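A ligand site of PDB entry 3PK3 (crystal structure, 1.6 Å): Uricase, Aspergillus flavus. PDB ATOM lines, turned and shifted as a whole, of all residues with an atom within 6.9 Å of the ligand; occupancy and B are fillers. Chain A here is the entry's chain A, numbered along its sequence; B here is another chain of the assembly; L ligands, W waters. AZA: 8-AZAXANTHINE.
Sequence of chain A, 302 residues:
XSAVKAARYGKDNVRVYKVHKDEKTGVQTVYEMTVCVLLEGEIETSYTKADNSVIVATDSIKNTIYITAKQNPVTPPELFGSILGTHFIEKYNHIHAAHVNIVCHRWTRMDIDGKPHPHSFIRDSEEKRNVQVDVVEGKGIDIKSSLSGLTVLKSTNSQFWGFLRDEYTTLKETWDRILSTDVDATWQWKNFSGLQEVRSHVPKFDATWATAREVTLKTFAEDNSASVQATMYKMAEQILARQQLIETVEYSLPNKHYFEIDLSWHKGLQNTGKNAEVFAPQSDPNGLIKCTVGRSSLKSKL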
ATOM      1  N   SER A 158      18.502 -17.282   0.937  1.00  0.00           N
ATOM      2  CA  SER A 158      18.980 -17.442  -0.424  1.00  0.00           C
ATOM      3  C   SER A 158      17.754 -17.719  -1.261  1.00  0.00           C
ATOM      4  O   SER A 158      16.877 -18.490  -0.852  1.00  0.00           O
ATOM      5  CB  SER A 158      19.980 -18.602  -0.536  1.00  0.00           C
ATOM      6  OG  SER A 158      20.273 -18.881  -1.908  1.00  0.00           O
ATOM      7  N   GLN A 159      17.697 -17.084  -2.428  1.00  0.00           N
ATOM      8  CA  GLN A 159      16.583 -17.223  -3.341  1.00  0.00           C
ATOM      9  C   GLN A 159      17.128 -17.467  -4.735  1.00  0.00           C
ATOM     10  O   GLN A 159      18.281 -17.144  -5.051  1.00  0.00           O
ATOM     11  CB  GLN A 159      15.745 -15.914  -3.388  1.00  0.00           C
ATOM     12  CG  GLN A 159      15.319 -15.444  -1.998  1.00  0.00           C
ATOM     13  CD  GLN A 159      14.404 -14.227  -2.031  1.00  0.00           C
ATOM     14  OE1 GLN A 159      14.125 -13.653  -3.076  1.00  0.00           O
ATOM     15  NE2 GLN A 159      13.931 -13.836  -0.852  1.00  0.00           N
ATOM     16  N   PHE A 160      16.288 -18.017  -5.589  1.00  0.00           N
ATOM     17  CA  PHE A 160      16.616 -18.081  -6.999  1.00  0.00           C
ATOM     18  C   PHE A 160      15.354 -18.194  -7.842  1.00  0.00           C
ATOM     19  O   PHE A 160      14.757 -19.261  -7.997  1.00  0.00           O
ATOM     20  CB  PHE A 160      17.629 -19.229  -7.311  1.00  0.00           C
ATOM     21  CG  PHE A 160      18.218 -19.143  -8.685  1.00  0.00           C
ATOM     22  CD1 PHE A 160      19.022 -18.047  -9.049  1.00  0.00           C
ATOM     23  CD2 PHE A 160      17.956 -20.118  -9.652  1.00  0.00           C
ATOM     24  CE1 PHE A 160      19.550 -17.930 -10.325  1.00  0.00           C
ATOM     25  CE2 PHE A 160      18.493 -20.029 -10.928  1.00  0.00           C
ATOM     26  CZ  PHE A 160      19.276 -18.912 -11.289  1.00  0.00           C
ATOM     27  N   PHE A 163      14.726 -16.686 -13.546  1.00  0.00           N
ATOM     28  CA  PHE A 163      15.621 -17.139 -14.599  1.00  0.00           C
ATOM     29  C   PHE A 163      14.891 -17.530 -15.891  1.00  0.00           C
ATOM     30  O   PHE A 163      13.666 -17.700 -15.881  1.00  0.00           O
ATOM     31  CB  PHE A 163      16.497 -18.305 -14.101  1.00  0.00           C
ATOM     32  CG  PHE A 163      15.718 -19.404 -13.427  1.00  0.00           C
ATOM     33  CD1 PHE A 163      15.479 -19.347 -12.048  1.00  0.00           C
ATOM     34  CD2 PHE A 163      15.229 -20.496 -14.168  1.00  0.00           C
ATOM     35  CE1 PHE A 163      14.758 -20.339 -11.392  1.00  0.00           C
ATOM     36  CE2 PHE A 163      14.506 -21.510 -13.506  1.00  0.00           C
ATOM     37  CZ  PHE A 163      14.259 -21.416 -12.134  1.00  0.00           C
ATOM     38  N   LEU A 171      13.639 -26.713 -13.507  1.00  0.00           N
ATOM     39  CA  LEU A 171      13.895 -26.148 -12.179  1.00  0.00           C
ATOM     40  C   LEU A 171      12.757 -25.225 -11.741  1.00  0.00           C
ATOM     41  O   LEU A 171      12.368 -24.320 -12.480  1.00  0.00           O
ATOM     42  CB  LEU A 171      15.205 -25.354 -12.224  1.00  0.00           C
ATOM     43  CG  LEU A 171      15.653 -24.722 -10.879  1.00  0.00           C
ATOM     44  CD1 LEU A 171      16.007 -25.820  -9.861  1.00  0.00           C
ATOM     45  CD2 LEU A 171      16.845 -23.790 -11.072  1.00  0.00           C
ATOM     46  N   ARG A 177      16.056 -21.196  -0.073  1.00  0.00           N
ATOM     47  CA  ARG A 177      16.825 -22.431  -0.313  1.00  0.00           C
ATOM     48  C   ARG A 177      18.097 -22.409   0.520  1.00  0.00           C
ATOM     49  O   ARG A 177      18.479 -21.377   1.089  1.00  0.00           O
ATOM     50  CB  ARG A 177      17.169 -22.568  -1.803  1.00  0.00           C
ATOM     51  CG  ARG A 177      18.110 -21.468  -2.282  1.00  0.00           C
ATOM     52  CD  ARG A 177      18.457 -21.649  -3.746  1.00  0.00           C
ATOM     53  NE  ARG A 177      19.513 -20.692  -4.112  1.00  0.00           N
ATOM     54  CZ  ARG A 177      20.185 -20.683  -5.262  1.00  0.00           C
ATOM     55  NH1 ARG A 177      19.918 -21.564  -6.247  1.00  0.00           N
ATOM     56  NH2 ARG A 177      21.130 -19.762  -5.452  1.00  0.00           N
ATOM     57  N   LEU A 179      22.109 -22.478   0.618  1.00  0.00           N
ATOM     58  CA  LEU A 179      23.245 -22.102  -0.228  1.00  0.00           C
ATOM     59  C   LEU A 179      24.544 -22.532   0.434  1.00  0.00           C
ATOM     60  O   LEU A 179      24.850 -22.140   1.560  1.00  0.00           O
ATOM     61  CB  LEU A 179      23.242 -20.584  -0.507  1.00  0.00           C
ATOM     62  CG  LEU A 179      24.349 -20.016  -1.384  1.00  0.00           C
ATOM     63  CD1 LEU A 179      24.283 -20.680  -2.748  1.00  0.00           C
ATOM     64  CD2 LEU A 179      24.115 -18.509  -1.548  1.00  0.00           C
ATOM     65  N   SER A 225      20.409 -13.388  -0.646  1.00  0.00           N
ATOM     66  CA  SER A 225      21.033 -13.619  -1.928  1.00  0.00           C
ATOM     67  C   SER A 225      20.047 -13.874  -3.066  1.00  0.00           C
ATOM     68  O   SER A 225      19.185 -14.747  -2.971  1.00  0.00           O
ATOM     69  CB  SER A 225      22.028 -14.786  -1.788  1.00  0.00           C
ATOM     70  OG  SER A 225      22.531 -15.151  -3.053  1.00  0.00           O
ATOM     71  N   ALA A 226      20.190 -13.111  -4.146  1.00  0.00           N
ATOM     72  CA  ALA A 226      19.333 -13.261  -5.300  1.00  0.00           C
ATOM     73  C   ALA A 226      19.856 -14.340  -6.223  1.00  0.00           C
ATOM     74  O   ALA A 226      19.135 -14.826  -7.098  1.00  0.00           O
ATOM     75  CB  ALA A 226      19.253 -11.920  -6.048  1.00  0.00           C
ATOM     76  N   SER A 227      21.136 -14.700  -6.026  1.00  0.00           N
ATOM     77  CA  SER A 227      21.825 -15.722  -6.859  1.00  0.00           C
ATOM     78  C   SER A 227      23.255 -15.760  -6.379  1.00  0.00           C
ATOM     79  O   SER A 227      23.718 -14.843  -5.675  1.00  0.00           O
ATOM     80  CB  SER A 227      21.827 -15.386  -8.370  1.00  0.00           C
ATOM     81  OG  SER A 227      22.593 -14.197  -8.650  1.00  0.00           O
ATOM     82  N   VAL A 228      24.005 -16.787  -6.786  1.00  0.00           N
ATOM     83  CA  VAL A 228      25.416 -16.830  -6.455  1.00  0.00           C
ATOM     84  C   VAL A 228      26.117 -15.652  -7.135  1.00  0.00           C
ATOM     85  O   VAL A 228      26.982 -15.010  -6.524  1.00  0.00           O
ATOM     86  CB  VAL A 228      26.024 -18.186  -6.904  1.00  0.00           C
ATOM     87  CG1 VAL A 228      27.532 -18.171  -6.730  1.00  0.00           C
ATOM     88  CG2 VAL A 228      25.408 -19.277  -6.041  1.00  0.00           C
ATOM     89  N   GLN A 229      25.728 -15.412  -8.374  1.00  0.00           N
ATOM     90  CA  GLN A 229      26.280 -14.342  -9.230  1.00  0.00           C
ATOM     91  C   GLN A 229      26.195 -13.002  -8.501  1.00  0.00           C
ATOM     92  O   GLN A 229      27.198 -12.254  -8.412  1.00  0.00           O
ATOM     93  CB  GLN A 229      25.482 -14.271 -10.534  1.00  0.00           C
ATOM     94  CG  GLN A 229      25.795 -15.376 -11.570  1.00  0.00           C
ATOM     95  CD  GLN A 229      24.949 -16.622 -11.405  1.00  0.00           C
ATOM     96  OE1 GLN A 229      24.447 -16.935 -10.315  1.00  0.00           O
ATOM     97  NE2 GLN A 229      24.822 -17.386 -12.498  1.00  0.00           N
ATOM     98  N   ALA A 230      25.007 -12.670  -7.997  1.00  0.00           N
ATOM     99  CA  ALA A 230      24.803 -11.350  -7.382  1.00  0.00           C
ATOM    100  C   ALA A 230      25.573 -11.188  -6.065  1.00  0.00           C
ATOM    101  O   ALA A 230      26.165 -10.127  -5.796  1.00  0.00           O
ATOM    102  CB  ALA A 230      23.306 -11.087  -7.204  1.00  0.00           C
ATOM    103  N   ASN A 255      28.180 -24.354  -6.647  1.00  0.00           N
ATOM    104  CA  ASN A 255      26.916 -24.307  -5.966  1.00  0.00           C
ATOM    105  C   ASN A 255      26.643 -25.745  -5.540  1.00  0.00           C
ATOM    106  O   ASN A 255      26.347 -26.564  -6.383  1.00  0.00           O
ATOM    107  CB  ASN A 255      25.869 -23.729  -6.918  1.00  0.00           C
ATOM    108  CG  ASN A 255      24.531 -23.462  -6.249  1.00  0.00           C
ATOM    109  OD1 ASN A 255      24.373 -23.629  -5.031  1.00  0.00           O
ATOM    110  ND2 ASN A 255      23.538 -23.042  -7.046  1.00  0.00           N
ATOM    111  N   HIS A 257      24.607 -28.438  -4.122  1.00  0.00           N
ATOM    112  CA  HIS A 257      23.153 -28.520  -3.990  1.00  0.00           C
ATOM    113  C   HIS A 257      22.699 -29.416  -2.863  1.00  0.00           C
ATOM    114  O   HIS A 257      23.252 -30.483  -2.655  1.00  0.00           O
ATOM    115  CB  HIS A 257      22.546 -29.004  -5.296  1.00  0.00           C
ATOM    116  CG  HIS A 257      22.970 -28.196  -6.485  1.00  0.00           C
ATOM    117  ND1 HIS A 257      22.592 -26.892  -6.670  1.00  0.00           N
ATOM    118  CD2 HIS A 257      23.757 -28.520  -7.540  1.00  0.00           C
ATOM    119  CE1 HIS A 257      23.099 -26.435  -7.809  1.00  0.00           C
ATOM    120  NE2 HIS A 257      23.828 -27.397  -8.347  1.00  0.00           N
ATOM    121  N   GLY A 287      26.668 -26.692  -9.734  1.00  0.00           N
ATOM    122  CA  GLY A 287      26.857 -25.421 -10.449  1.00  0.00           C
ATOM    123  C   GLY A 287      28.275 -24.919 -10.232  1.00  0.00           C
ATOM    124  O   GLY A 287      28.931 -25.232  -9.242  1.00  0.00           O
ATOM    125  N   ILE A 289      30.243 -21.184 -10.795  1.00  0.00           N
ATOM    126  CA  ILE A 289      30.002 -19.785 -11.177  1.00  0.00           C
ATOM    127  C   ILE A 289      31.291 -19.011 -10.988  1.00  0.00           C
ATOM    128  O   ILE A 289      31.893 -19.060  -9.908  1.00  0.00           O
ATOM    129  CB  ILE A 289      28.924 -19.132 -10.247  1.00  0.00           C
ATOM    130  CG1 ILE A 289      27.713 -20.080 -10.015  1.00  0.00           C
ATOM    131  CG2 ILE A 289      28.476 -17.774 -10.851  1.00  0.00           C
ATOM    132  CD1 ILE A 289      26.982 -20.511 -11.216  1.00  0.00           C
ATOM    133  N   TYR B   9      29.772 -19.285 -16.334  1.00  0.00           N
ATOM    134  CA  TYR B   9      29.061 -20.064 -15.323  1.00  0.00           C
ATOM    135  C   TYR B   9      28.471 -21.290 -16.043  1.00  0.00           C
ATOM    136  O   TYR B   9      28.300 -21.288 -17.270  1.00  0.00           O
ATOM    137  CB  TYR B   9      27.997 -19.199 -14.625  1.00  0.00           C
ATOM    138  CG  TYR B   9      26.752 -19.166 -15.434  1.00  0.00           C
ATOM    139  CD1 TYR B   9      26.691 -18.452 -16.619  1.00  0.00           C
ATOM    140  CD2 TYR B   9      25.664 -19.966 -15.094  1.00  0.00           C
ATOM    141  CE1 TYR B   9      25.557 -18.511 -17.430  1.00  0.00           C
ATOM    142  CE2 TYR B   9      24.542 -20.021 -15.867  1.00  0.00           C
ATOM    143  CZ  TYR B   9      24.501 -19.279 -17.046  1.00  0.00           C
ATOM    144  OH  TYR B   9      23.393 -19.340 -17.837  1.00  0.00           O
ATOM    145  N   GLY B  10      28.142 -22.330 -15.266  1.00  0.00           N
ATOM    146  CA  GLY B  10      27.504 -23.493 -15.849  1.00  0.00           C
ATOM    147  C   GLY B  10      27.479 -24.653 -14.888  1.00  0.00           C
ATOM    148  O   GLY B  10      27.370 -24.465 -13.713  1.00  0.00           O
ATOM    149  N   LYS B  11      27.605 -25.864 -15.413  1.00  0.00           N
ATOM    150  CA  LYS B  11      27.432 -27.066 -14.568  1.00  0.00           C
ATOM    151  C   LYS B  11      28.679 -27.923 -14.703  1.00  0.00           C
ATOM    152  O   LYS B  11      29.164 -28.140 -15.820  1.00  0.00           O
ATOM    153  CB  LYS B  11      26.208 -27.875 -15.013  1.00  0.00           C
ATOM    154  CG  LYS B  11      25.714 -28.852 -13.944  1.00  0.00           C
ATOM    155  CD  LYS B  11      25.180 -28.094 -12.729  1.00  0.00           C
ATOM    156  CE  LYS B  11      23.780 -28.453 -12.361  1.00  0.00           C
ATOM    157  NZ  LYS B  11      23.204 -27.491 -11.354  1.00  0.00           N
ATOM    158  N   ASN B  52      18.138 -12.027 -13.123  1.00  0.00           N
ATOM    159  CA  ASN B  52      18.227 -13.437 -13.501  1.00  0.00           C
ATOM    160  C   ASN B  52      17.683 -13.790 -14.888  1.00  0.00           C
ATOM    161  O   ASN B  52      17.825 -14.927 -15.340  1.00  0.00           O
ATOM    162  CB  ASN B  52      17.626 -14.337 -12.400  1.00  0.00           C
ATOM    163  CG  ASN B  52      18.430 -14.287 -11.110  1.00  0.00           C
ATOM    164  OD1 ASN B  52      19.619 -13.967 -11.128  1.00  0.00           O
ATOM    165  ND2 ASN B  52      17.796 -14.607  -9.984  1.00  0.00           N
ATOM    166  N   ILE B  55      19.955 -15.572 -17.234  1.00  0.00           N
ATOM    167  CA  ILE B  55      20.550 -16.850 -16.825  1.00  0.00           C
ATOM    168  C   ILE B  55      19.805 -18.071 -17.347  1.00  0.00           C
ATOM    169  O   ILE B  55      18.634 -18.281 -17.029  1.00  0.00           O
ATOM    170  CB  ILE B  55      20.662 -16.961 -15.291  1.00  0.00           C
ATOM    171  CG1 ILE B  55      21.558 -15.851 -14.720  1.00  0.00           C
ATOM    172  CG2 ILE B  55      21.248 -18.358 -14.898  1.00  0.00           C
ATOM    173  CD1 ILE B  55      21.525 -15.806 -13.166  1.00  0.00           C
ATOM    174  N   VAL B  56      20.496 -18.861 -18.159  1.00  0.00           N
ATOM    175  CA  VAL B  56      20.057 -20.210 -18.505  1.00  0.00           C
ATOM    176  C   VAL B  56      20.468 -21.004 -17.247  1.00  0.00           C
ATOM    177  O   VAL B  56      21.664 -21.084 -16.966  1.00  0.00           O
ATOM    178  CB  VAL B  56      20.771 -20.726 -19.768  1.00  0.00           C
ATOM    179  CG1 VAL B  56      20.408 -22.200 -20.053  1.00  0.00           C
ATOM    180  CG2 VAL B  56      20.414 -19.837 -20.980  1.00  0.00           C
ATOM    181  N   ALA B  57      19.500 -21.532 -16.489  1.00  0.00           N
ATOM    182  CA  ALA B  57      19.825 -22.163 -15.191  1.00  0.00           C
ATOM    183  C   ALA B  57      20.812 -23.312 -15.385  1.00  0.00           C
ATOM    184  O   ALA B  57      20.770 -24.010 -16.397  1.00  0.00           O
ATOM    185  CB  ALA B  57      18.552 -22.657 -14.484  1.00  0.00           C
ATOM    186  N   THR B  58      21.711 -23.478 -14.413  1.00  0.00           N
ATOM    187  CA  THR B  58      22.733 -24.518 -14.521  1.00  0.00           C
ATOM    188  C   THR B  58      22.010 -25.868 -14.552  1.00  0.00           C
ATOM    189  O   THR B  58      22.443 -26.797 -15.233  1.00  0.00           O
ATOM    190  CB  THR B  58      23.785 -24.463 -13.379  1.00  0.00           C
ATOM    191  OG1 THR B  58      23.166 -24.761 -12.133  1.00  0.00           O
ATOM    192  CG2 THR B  58      24.467 -23.077 -13.348  1.00  0.00           C
ATOM    193  N   ASP B  59      20.886 -25.946 -13.825  1.00  0.00           N
ATOM    194  CA  ASP B  59      20.027 -27.144 -13.870  1.00  0.00           C
ATOM    195  C   ASP B  59      19.566 -27.466 -15.309  1.00  0.00           C
ATOM    196  O   ASP B  59      19.511 -28.632 -15.705  1.00  0.00           O
ATOM    197  CB  ASP B  59      18.832 -27.028 -12.938  1.00  0.00           C
ATOM    198  CG  ASP B  59      18.092 -28.345 -12.797  1.00  0.00           C
ATOM    199  OD1 ASP B  59      18.567 -29.210 -12.022  1.00  0.00           O
ATOM    200  OD2 ASP B  59      17.047 -28.527 -13.465  1.00  0.00           O
ATOM    201  N   SER B  60      19.228 -26.426 -16.080  1.00  0.00           N
ATOM    202  CA  SER B  60      18.834 -26.609 -17.483  1.00  0.00           C
ATOM    203  C   SER B  60      19.988 -27.039 -18.354  1.00  0.00           C
ATOM    204  O   SER B  60      19.809 -27.790 -19.306  1.00  0.00           O
ATOM    205  CB  SER B  60      18.212 -25.314 -18.048  1.00  0.00           C
ATOM    206  OG  SER B  60      17.184 -24.892 -17.186  1.00  0.00           O
HETATM  207  N1  AZA L   1      22.836 -19.379  -9.971  1.00  0.00           N
HETATM  208  C2  AZA L   1      22.311 -19.781  -8.789  1.00  0.00           C
HETATM  209  O2  AZA L   1      22.550 -19.084  -7.792  1.00  0.00           O
HETATM  210  N3  AZA L   1      21.519 -20.912  -8.664  1.00  0.00           N
HETATM  211  C4  AZA L   1      21.229 -21.631  -9.761  1.00  0.00           C
HETATM  212  C5  AZA L   1      21.789 -21.244 -11.059  1.00  0.00           C
HETATM  213  C6  AZA L   1      22.631 -20.039 -11.119  1.00  0.00           C
HETATM  214  O6  AZA L   1      23.133 -19.678 -12.199  1.00  0.00           O
HETATM  215  N7  AZA L   1      21.360 -22.105 -11.999  1.00  0.00           N
HETATM  216  N8  AZA L   1      20.579 -23.033 -11.345  1.00  0.00           N
HETATM  217  N9  AZA L   1      20.504 -22.735  -9.989  1.00  0.00           N
HETATM  218  O   HOH W   1      19.490 -24.393  -8.071  1.00  0.00           O
HETATM  219  O   HOH W   2      24.161 -23.524  -9.851  1.00  0.00           O
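The backbone NH of Arg 177 sits at hydrogen-bond distance from the backbone carbonyl oxygen of Ser 158, 2.9 Å away.
The side-chain hydroxyl of Thr 58 of chain B lies within hydrogen-bond range of the side-chain amino group of Lys 11 of chain B (2.8 Å).
The backbone carbonyl oxygen (O) of Ser 227 is in hydrogen-bond range of the side-chain hydroxyl (OG) of Ser 225, 2.9 Å away.
The backbone NH of Asn 255 lies within hydrogen-bond range of the backbone carbonyl oxygen of Gly 287 (2.8 Å).
The backbone carbonyl oxygen of Asn 255 is in hydrogen-bond range of a ring nitrogen (NE2) of His 257, at 3.3 Å.
The backbone carbonyl oxygen (O) of Val 56 of chain B is in hydrogen-bond range of the side-chain hydroxyl (OH) of Tyr 9 of chain B (2.6 Å).
N of Gln 229 lies close to OG of Ser 227 (3.4 Å).
The backbone NH (N) of Ala 230 sits at hydrogen-bond distance from the side-chain hydroxyl (OG) of Ser 227 (2.9 Å).
Residues that only touch the ligand: Phe 160, Leu 171, Ser 227, Tyr 9 of chain B, Ile 55 of chain B, Ala 57 of chain B and Asp 59 of chain B.
Hydrophobic or aromatic side chains that line the ligand: Phe 160, Leu 171, Val 228, Tyr 9 of chain B, Ile 55 of chain B and Ala 57 of chain B.
12 residues have an atom within 4 Å of the ligand: Phe 160, Leu 171, Arg 177, Ser 227, Val 228, Gln 229, Asn 255, Tyr 9 of chain B, Ile 55 of chain B, Ala 57 of chain B, Thr 58 of chain B and Asp 59 of chain B.
Water W1 lies within hydrogen-bond range of N9 of the ligand (2.7 Å) and NH1 of Arg 177 (3.4 Å).
Water W2 bridges the side-chain hydroxyl (OG1) of Thr 58 of chain B (2.8 Å) and the side-chain amide nitrogen (ND2) of Asn 255 (2.9 Å).
The side-chain amide nitrogen (NE2) of Gln 229 is in hydrogen-bond range of an oxygen (O6) of the ligand (2.9 Å).
N of Val 228 sits at hydrogen-bond distance from O2 of the ligand.
The backbone NH (N) of Thr 58 of chain B lies within hydrogen-bond range of a nitrogen (N7) of the ligand (2.8 Å).
O2 of the ligand is in hydrogen-bond range of NH2 of Arg 177, at 2.8 Å.
A nitrogen (N8) of the ligand lies within hydrogen-bond range of the side-chain hydroxyl of Thr 58 of chain B.
The side-chain amide nitrogen of Asn 255 sits close to a nitrogen (N3) of the ligand (3.4 Å).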
